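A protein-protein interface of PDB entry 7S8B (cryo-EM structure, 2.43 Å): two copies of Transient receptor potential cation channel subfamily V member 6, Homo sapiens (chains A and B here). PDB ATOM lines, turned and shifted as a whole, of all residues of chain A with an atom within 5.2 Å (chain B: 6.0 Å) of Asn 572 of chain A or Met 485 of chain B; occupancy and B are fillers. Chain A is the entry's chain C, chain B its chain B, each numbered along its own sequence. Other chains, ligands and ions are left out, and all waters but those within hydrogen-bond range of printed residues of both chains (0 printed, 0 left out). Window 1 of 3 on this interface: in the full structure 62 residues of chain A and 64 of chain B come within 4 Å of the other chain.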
ATOM      1  N   THR A 567       3.636 -13.388   6.042  1.00  0.00           N
ATOM      2  CA  THR A 567       3.299 -13.816   7.396  1.00  0.00           C
ATOM      3  C   THR A 567       2.064 -14.715   7.442  1.00  0.00           C
ATOM      4  O   THR A 567       1.991 -15.577   8.319  1.00  0.00           O
ATOM      5  CB  THR A 567       3.093 -12.622   8.320  1.00  0.00           C
ATOM      6  OG1 THR A 567       1.946 -11.880   7.896  1.00  0.00           O
ATOM      7  CG2 THR A 567       4.330 -11.728   8.321  1.00  0.00           C
ATOM      8  N   LEU A 568       1.088 -14.515   6.544  1.00  0.00           N
ATOM      9  CA  LEU A 568       0.027 -15.501   6.306  1.00  0.00           C
ATOM     10  C   LEU A 568       0.587 -16.877   5.993  1.00  0.00           C
ATOM     11  O   LEU A 568       0.191 -17.870   6.610  1.00  0.00           O
ATOM     12  CB  LEU A 568      -0.866 -15.060   5.145  1.00  0.00           C
ATOM     13  CG  LEU A 568      -1.821 -16.110   4.545  1.00  0.00           C
ATOM     14  CD1 LEU A 568      -2.940 -16.538   5.484  1.00  0.00           C
ATOM     15  CD2 LEU A 568      -2.381 -15.666   3.207  1.00  0.00           C
ATOM     16  N   LEU A 569       1.500 -16.952   5.022  1.00  0.00           N
ATOM     17  CA  LEU A 569       2.091 -18.226   4.639  1.00  0.00           C
ATOM     18  C   LEU A 569       2.946 -18.813   5.751  1.00  0.00           C
ATOM     19  O   LEU A 569       2.883 -20.019   5.999  1.00  0.00           O
ATOM     20  CB  LEU A 569       2.912 -18.074   3.362  1.00  0.00           C
ATOM     21  CG  LEU A 569       2.098 -17.914   2.085  1.00  0.00           C
ATOM     22  CD1 LEU A 569       2.990 -17.708   0.892  1.00  0.00           C
ATOM     23  CD2 LEU A 569       1.238 -19.126   1.884  1.00  0.00           C
ATOM     24  N   MET A 570       3.744 -17.983   6.429  1.00  0.00           N
ATOM     25  CA  MET A 570       4.599 -18.473   7.507  1.00  0.00           C
ATOM     26  C   MET A 570       3.780 -19.022   8.666  1.00  0.00           C
ATOM     27  O   MET A 570       4.118 -20.066   9.231  1.00  0.00           O
ATOM     28  CB  MET A 570       5.530 -17.364   7.995  1.00  0.00           C
ATOM     29  CG  MET A 570       6.474 -17.787   9.089  1.00  0.00           C
ATOM     30  SD  MET A 570       7.588 -16.491   9.668  1.00  0.00           S
ATOM     31  CE  MET A 570       8.773 -16.462   8.332  1.00  0.00           C
ATOM     32  N   LEU A 571       2.679 -18.356   9.008  1.00  0.00           N
ATOM     33  CA  LEU A 571       1.794 -18.887  10.032  1.00  0.00           C
ATOM     34  C   LEU A 571       1.002 -20.090   9.545  1.00  0.00           C
ATOM     35  O   LEU A 571       0.500 -20.842  10.373  1.00  0.00           O
ATOM     36  CB  LEU A 571       0.845 -17.806  10.532  1.00  0.00           C
ATOM     37  CG  LEU A 571       1.459 -16.679  11.354  1.00  0.00           C
ATOM     38  CD1 LEU A 571       0.420 -15.657  11.690  1.00  0.00           C
ATOM     39  CD2 LEU A 571       2.076 -17.218  12.602  1.00  0.00           C
ATOM     40  N   ASN A 572       0.886 -20.289   8.230  1.00  0.00           N
ATOM     41  CA  ASN A 572       0.246 -21.473   7.671  1.00  0.00           C
ATOM     42  C   ASN A 572       1.178 -22.681   7.682  1.00  0.00           C
ATOM     43  O   ASN A 572       0.713 -23.814   7.822  1.00  0.00           O
ATOM     44  CB  ASN A 572      -0.203 -21.195   6.242  1.00  0.00           C
ATOM     45  CG  ASN A 572      -1.157 -22.239   5.707  1.00  0.00           C
ATOM     46  OD1 ASN A 572      -1.656 -23.094   6.440  1.00  0.00           O
ATOM     47  ND2 ASN A 572      -1.424 -22.172   4.415  1.00  0.00           N
ATOM     48  N   LEU A 573       2.483 -22.469   7.504  1.00  0.00           N
ATOM     49  CA  LEU A 573       3.439 -23.558   7.678  1.00  0.00           C
ATOM     50  C   LEU A 573       3.449 -24.059   9.113  1.00  0.00           C
ATOM     51  O   LEU A 573       3.622 -25.257   9.359  1.00  0.00           O
ATOM     52  CB  LEU A 573       4.835 -23.100   7.261  1.00  0.00           C
ATOM     53  CG  LEU A 573       5.969 -24.101   7.431  1.00  0.00           C
ATOM     54  CD1 LEU A 573       5.670 -25.364   6.635  1.00  0.00           C
ATOM     55  CD2 LEU A 573       7.285 -23.500   7.012  1.00  0.00           C
ATOM     56  N   LEU A 574       3.224 -23.159  10.059  1.00  0.00           N
ATOM     57  CA  LEU A 574       3.166 -23.515  11.463  1.00  0.00           C
ATOM     58  C   LEU A 574       1.948 -24.378  11.762  1.00  0.00           C
ATOM     59  O   LEU A 574       1.993 -25.215  12.669  1.00  0.00           O
ATOM     60  CB  LEU A 574       3.150 -22.225  12.270  1.00  0.00           C
ATOM     61  CG  LEU A 574       3.570 -22.110  13.725  1.00  0.00           C
ATOM     62  CD1 LEU A 574       3.709 -20.633  13.979  1.00  0.00           C
ATOM     63  CD2 LEU A 574       2.588 -22.701  14.677  1.00  0.00           C
ATOM     64  N   ILE A 575       0.852 -24.157  11.030  1.00  0.00           N
ATOM     65  CA  ILE A 575      -0.321 -25.022  11.102  1.00  0.00           C
ATOM     66  C   ILE A 575       0.041 -26.429  10.681  1.00  0.00           C
ATOM     67  O   ILE A 575      -0.146 -27.394  11.429  1.00  0.00           O
ATOM     68  CB  ILE A 575      -1.437 -24.517  10.176  1.00  0.00           C
ATOM     69  CG1 ILE A 575      -1.794 -23.050  10.371  1.00  0.00           C
ATOM     70  CG2 ILE A 575      -2.582 -25.466  10.239  1.00  0.00           C
ATOM     71  CD1 ILE A 575      -2.047 -22.650  11.706  1.00  0.00           C
ATOM     72  N   ALA A 576       0.532 -26.555   9.443  1.00  0.00           N
ATOM     73  CA  ALA A 576       0.680 -27.842   8.784  1.00  0.00           C
ATOM     74  C   ALA A 576       1.688 -28.720   9.493  1.00  0.00           C
ATOM     75  O   ALA A 576       1.561 -29.947   9.471  1.00  0.00           O
ATOM     76  CB  ALA A 576       1.084 -27.633   7.326  1.00  0.00           C
ATOM     77  N   PHE B 478      -3.184 -28.336   0.738  1.00  0.00           N
ATOM     78  CA  PHE B 478      -2.526 -27.214   1.392  1.00  0.00           C
ATOM     79  C   PHE B 478      -2.971 -25.882   0.802  1.00  0.00           C
ATOM     80  O   PHE B 478      -3.086 -24.887   1.521  1.00  0.00           O
ATOM     81  CB  PHE B 478      -1.008 -27.380   1.302  1.00  0.00           C
ATOM     82  CG  PHE B 478      -0.243 -26.226   1.866  1.00  0.00           C
ATOM     83  CD1 PHE B 478      -0.246 -25.970   3.229  1.00  0.00           C
ATOM     84  CD2 PHE B 478       0.495 -25.406   1.039  1.00  0.00           C
ATOM     85  CE1 PHE B 478       0.460 -24.894   3.750  1.00  0.00           C
ATOM     86  CE2 PHE B 478       1.211 -24.340   1.551  1.00  0.00           C
ATOM     87  CZ  PHE B 478       1.186 -24.083   2.911  1.00  0.00           C
ATOM     88  N   ILE B 480      -5.890 -25.043  -0.501  1.00  0.00           N
ATOM     89  CA  ILE B 480      -7.238 -24.674  -0.063  1.00  0.00           C
ATOM     90  C   ILE B 480      -7.200 -24.013   1.312  1.00  0.00           C
ATOM     91  O   ILE B 480      -7.990 -23.104   1.604  1.00  0.00           O
ATOM     92  CB  ILE B 480      -8.144 -25.918  -0.063  1.00  0.00           C
ATOM     93  CG1 ILE B 480      -8.169 -26.548  -1.446  1.00  0.00           C
ATOM     94  CG2 ILE B 480      -9.578 -25.576   0.322  1.00  0.00           C
ATOM     95  CD1 ILE B 480      -8.821 -27.854  -1.450  1.00  0.00           C
ATOM     96  N   MET B 481      -6.286 -24.467   2.177  1.00  0.00           N
ATOM     97  CA  MET B 481      -6.077 -23.849   3.485  1.00  0.00           C
ATOM     98  C   MET B 481      -5.715 -22.371   3.369  1.00  0.00           C
ATOM     99  O   MET B 481      -6.091 -21.571   4.229  1.00  0.00           O
ATOM    100  CB  MET B 481      -4.988 -24.605   4.233  1.00  0.00           C
ATOM    101  CG  MET B 481      -5.358 -26.023   4.564  1.00  0.00           C
ATOM    102  SD  MET B 481      -3.971 -26.993   5.183  1.00  0.00           S
ATOM    103  CE  MET B 481      -3.696 -26.249   6.783  1.00  0.00           C
ATOM    104  N   ILE B 482      -5.008 -21.993   2.302  1.00  0.00           N
ATOM    105  CA  ILE B 482      -4.609 -20.605   2.096  1.00  0.00           C
ATOM    106  C   ILE B 482      -5.824 -19.717   1.851  1.00  0.00           C
ATOM    107  O   ILE B 482      -5.940 -18.632   2.434  1.00  0.00           O
ATOM    108  CB  ILE B 482      -3.599 -20.523   0.938  1.00  0.00           C
ATOM    109  CG1 ILE B 482      -2.300 -21.244   1.303  1.00  0.00           C
ATOM    110  CG2 ILE B 482      -3.308 -19.092   0.559  1.00  0.00           C
ATOM    111  CD1 ILE B 482      -1.401 -21.472   0.122  1.00  0.00           C
ATOM    112  N   GLN B 483      -6.766 -20.180   1.024  1.00  0.00           N
ATOM    113  CA  GLN B 483      -7.961 -19.404   0.708  1.00  0.00           C
ATOM    114  C   GLN B 483      -8.858 -19.220   1.922  1.00  0.00           C
ATOM    115  O   GLN B 483      -9.378 -18.124   2.160  1.00  0.00           O
ATOM    116  CB  GLN B 483      -8.749 -20.097  -0.391  1.00  0.00           C
ATOM    117  CG  GLN B 483     -10.055 -19.434  -0.738  1.00  0.00           C
ATOM    118  CD  GLN B 483     -10.878 -20.266  -1.678  1.00  0.00           C
ATOM    119  OE1 GLN B 483     -10.486 -21.363  -2.056  1.00  0.00           O
ATOM    120  NE2 GLN B 483     -12.049 -19.756  -2.048  1.00  0.00           N
ATOM    121  N   LYS B 484      -9.046 -20.270   2.705  1.00  0.00           N
ATOM    122  CA  LYS B 484      -9.993 -20.190   3.798  1.00  0.00           C
ATOM    123  C   LYS B 484      -9.444 -19.448   5.001  1.00  0.00           C
ATOM    124  O   LYS B 484     -10.215 -19.105   5.900  1.00  0.00           O
ATOM    125  CB  LYS B 484     -10.452 -21.584   4.178  1.00  0.00           C
ATOM    126  CG  LYS B 484     -11.357 -22.189   3.113  1.00  0.00           C
ATOM    127  CD  LYS B 484     -11.804 -23.568   3.501  1.00  0.00           C
ATOM    128  CE  LYS B 484     -12.658 -24.200   2.425  1.00  0.00           C
ATOM    129  NZ  LYS B 484     -13.972 -23.516   2.304  1.00  0.00           N
ATOM    130  N   MET B 485      -8.149 -19.168   5.033  1.00  0.00           N
ATOM    131  CA  MET B 485      -7.643 -18.296   6.072  1.00  0.00           C
ATOM    132  C   MET B 485      -7.514 -16.851   5.635  1.00  0.00           C
ATOM    133  O   MET B 485      -7.598 -15.974   6.493  1.00  0.00           O
ATOM    134  CB  MET B 485      -6.309 -18.805   6.599  1.00  0.00           C
ATOM    135  CG  MET B 485      -6.471 -20.113   7.320  1.00  0.00           C
ATOM    136  SD  MET B 485      -4.933 -20.615   8.058  1.00  0.00           S
ATOM    137  CE  MET B 485      -4.003 -20.662   6.560  1.00  0.00           C
ATOM    138  N   ILE B 486      -7.352 -16.567   4.341  1.00  0.00           N
ATOM    139  CA  ILE B 486      -7.330 -15.166   3.929  1.00  0.00           C
ATOM    140  C   ILE B 486      -8.736 -14.572   3.941  1.00  0.00           C
ATOM    141  O   ILE B 486      -8.930 -13.436   4.385  1.00  0.00           O
ATOM    142  CB  ILE B 486      -6.599 -14.970   2.580  1.00  0.00           C
ATOM    143  CG1 ILE B 486      -6.510 -13.483   2.247  1.00  0.00           C
ATOM    144  CG2 ILE B 486      -7.234 -15.714   1.442  1.00  0.00           C
ATOM    145  CD1 ILE B 486      -5.396 -13.102   1.311  1.00  0.00           C
ATOM    146  N   PHE B 487      -9.745 -15.324   3.514  1.00  0.00           N
ATOM    147  CA  PHE B 487     -11.101 -14.806   3.547  1.00  0.00           C
ATOM    148  C   PHE B 487     -11.807 -15.150   4.846  1.00  0.00           C
ATOM    149  O   PHE B 487     -13.013 -14.937   4.964  1.00  0.00           O
ATOM    150  CB  PHE B 487     -11.899 -15.302   2.339  1.00  0.00           C
ATOM    151  CG  PHE B 487     -11.403 -14.752   1.039  1.00  0.00           C
ATOM    152  CD1 PHE B 487     -11.623 -13.425   0.707  1.00  0.00           C
ATOM    153  CD2 PHE B 487     -10.721 -15.559   0.145  1.00  0.00           C
ATOM    154  CE1 PHE B 487     -11.159 -12.915  -0.490  1.00  0.00           C
ATOM    155  CE2 PHE B 487     -10.257 -15.058  -1.046  1.00  0.00           C
ATOM    156  CZ  PHE B 487     -10.478 -13.736  -1.367  1.00  0.00           C
ATOM    157  N   GLY B 488     -11.080 -15.692   5.809  1.00  0.00           N
ATOM    158  CA  GLY B 488     -11.566 -15.842   7.155  1.00  0.00           C
ATOM    159  C   GLY B 488     -10.697 -15.075   8.122  1.00  0.00           C
ATOM    160  O   GLY B 488     -10.860 -13.869   8.309  1.00  0.00           O
ATOM    161  N   ASP B 489      -9.742 -15.784   8.713  1.00  0.00           N
ATOM    162  CA  ASP B 489      -9.018 -15.283   9.872  1.00  0.00           C
ATOM    163  C   ASP B 489      -7.998 -14.205   9.541  1.00  0.00           C
ATOM    164  O   ASP B 489      -7.624 -13.433  10.429  1.00  0.00           O
ATOM    165  CB  ASP B 489      -8.356 -16.445  10.581  1.00  0.00           C
ATOM    166  CG  ASP B 489      -9.344 -17.262  11.359  1.00  0.00           C
ATOM    167  OD1 ASP B 489     -10.279 -16.706  11.972  1.00  0.00           O
ATOM    168  OD2 ASP B 489      -9.234 -18.486  11.313  1.00  0.00           O
ATOM    169  N   LEU B 490      -7.480 -14.157   8.313  1.00  0.00           N
ATOM    170  CA  LEU B 490      -6.547 -13.080   7.999  1.00  0.00           C
ATOM    171  C   LEU B 490      -7.279 -11.764   7.835  1.00  0.00           C
ATOM    172  O   LEU B 490      -6.829 -10.736   8.345  1.00  0.00           O
ATOM    173  CB  LEU B 490      -5.735 -13.396   6.747  1.00  0.00           C
ATOM    174  CG  LEU B 490      -4.630 -12.432   6.331  1.00  0.00           C
ATOM    175  CD1 LEU B 490      -3.540 -12.386   7.368  1.00  0.00           C
ATOM    176  CD2 LEU B 490      -4.069 -12.845   4.995  1.00  0.00           C
ATOM    177  N   MET B 491      -8.414 -11.782   7.130  1.00  0.00           N
ATOM    178  CA  MET B 491      -9.237 -10.592   6.972  1.00  0.00           C
ATOM    179  C   MET B 491      -9.852 -10.178   8.298  1.00  0.00           C
ATOM    180  O   MET B 491     -10.012  -8.984   8.575  1.00  0.00           O
ATOM    181  CB  MET B 491     -10.309 -10.863   5.913  1.00  0.00           C
ATOM    182  CG  MET B 491     -11.361  -9.790   5.710  1.00  0.00           C
ATOM    183  SD  MET B 491     -12.308 -10.050   4.194  1.00  0.00           S
ATOM    184  CE  MET B 491     -13.186 -11.574   4.537  1.00  0.00           C
ATOM    185  N   MET B 577      -5.802 -19.334  13.338  1.00  0.00           N
ATOM    186  CA  MET B 577      -5.456 -20.208  12.235  1.00  0.00           C
ATOM    187  C   MET B 577      -5.329 -21.668  12.651  1.00  0.00           C
ATOM    188  O   MET B 577      -5.298 -22.534  11.777  1.00  0.00           O
ATOM    189  CB  MET B 577      -4.160 -19.745  11.586  1.00  0.00           C
ATOM    190  CG  MET B 577      -4.259 -18.431  10.860  1.00  0.00           C
ATOM    191  SD  MET B 577      -2.720 -18.082  10.009  1.00  0.00           S
ATOM    192  CE  MET B 577      -3.127 -16.528   9.233  1.00  0.00           C
ATOM    193  N   ASP B 580      -9.019 -22.810  12.925  1.00  0.00           N
ATOM    194  CA  ASP B 580      -9.597 -22.792  11.588  1.00  0.00           C
ATOM    195  C   ASP B 580      -9.308 -24.083  10.858  1.00  0.00           C
ATOM    196  O   ASP B 580     -10.152 -24.593  10.117  1.00  0.00           O
ATOM    197  CB  ASP B 580      -9.040 -21.622  10.785  1.00  0.00           C
ATOM    198  CG  ASP B 580      -9.884 -21.274   9.571  1.00  0.00           C
ATOM    199  OD1 ASP B 580     -10.921 -21.926   9.318  1.00  0.00           O
ATOM    200  OD2 ASP B 580      -9.514 -20.314   8.869  1.00  0.00           O
ATOM    201  N   THR B 581      -8.111 -24.616  11.031  1.00  0.00           N
ATOM    202  CA  THR B 581      -7.723 -25.745  10.210  1.00  0.00           C
ATOM    203  C   THR B 581      -8.116 -27.058  10.858  1.00  0.00           C
ATOM    204  O   THR B 581      -8.975 -27.776  10.337  1.00  0.00           O
ATOM    205  CB  THR B 581      -6.226 -25.705   9.957  1.00  0.00           C
ATOM    206  OG1 THR B 581      -5.560 -25.712  11.216  1.00  0.00           O
ATOM    207  CG2 THR B 581      -5.886 -24.441   9.180  1.00  0.00           C
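The backbone carbonyl oxygen of Met 485 of chain B lies within hydrogen-bond range of the backbone NH of Leu 490 of chain B (2.6 Å). The side-chain hydroxyl of Thr 581 of chain B sits at hydrogen-bond distance from the backbone carbonyl oxygen of Met 577 of chain B, at 3.2 Å.
Leu 568 of chain A touches Leu 490 of chain B (CD2 to CD2, 3.7 Å). Leu 568 of chain A touches Met 577 of chain B. Ile 482 of chain B touches Leu 569 of chain A (CD1 to CD2, 3.9 Å). CB of Leu 571 of chain A touches SD of Met 577 of chain B, at 3.6 Å. Asn 572 of chain A touches Phe 478 of chain B. ND2 of Asn 572 of chain A touches CG1 of Ile 482 of chain B, 3.4 Å away. Met 485 of chain B touches Asn 572 of chain A. Met 481 of chain B touches Ile 575 of chain A. Met 577 of chain B touches Ile 575 of chain A. Thr 581 of chain B touches Ile 575 of chain A.
Printed residues of chain B within 4 Å of Leu 569 of chain A: Ile 482. Of the printed residues of chain B, Leu 571 of chain A touches Met 577 (3.6 Å). Of the printed residues of chain B, Asn 572 of chain A touches Phe 478 (3.4 Å), Met 481 (3.8 Å), Ile 482 (3.4 Å) and Met 485 (3.4 Å). Met 485 of chain B touches one residue of chain A. Asp 580 of chain B touches none of the printed residues of chain A. The nearest residue of chain A that does not touch Met 485 of chain B is Leu 568 of chain A (4.2 Å). The nearest printed residue of chain B that does not touch Leu 571 of chain A is Met 485 of chain B (5.9 Å).
Hydrophobic or aromatic side chains of chain A within 4 Å of the printed part of chain B: Leu 568, Leu 569, Leu 571 and Ile 575. Of the 16 printed residues of chain B, 7 touch a printed residue of chain A.
No position is printed for both chains. Of the 11 pairs that touch across the chains among the printed residues, none has its exchanged pair printed and touching as well.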
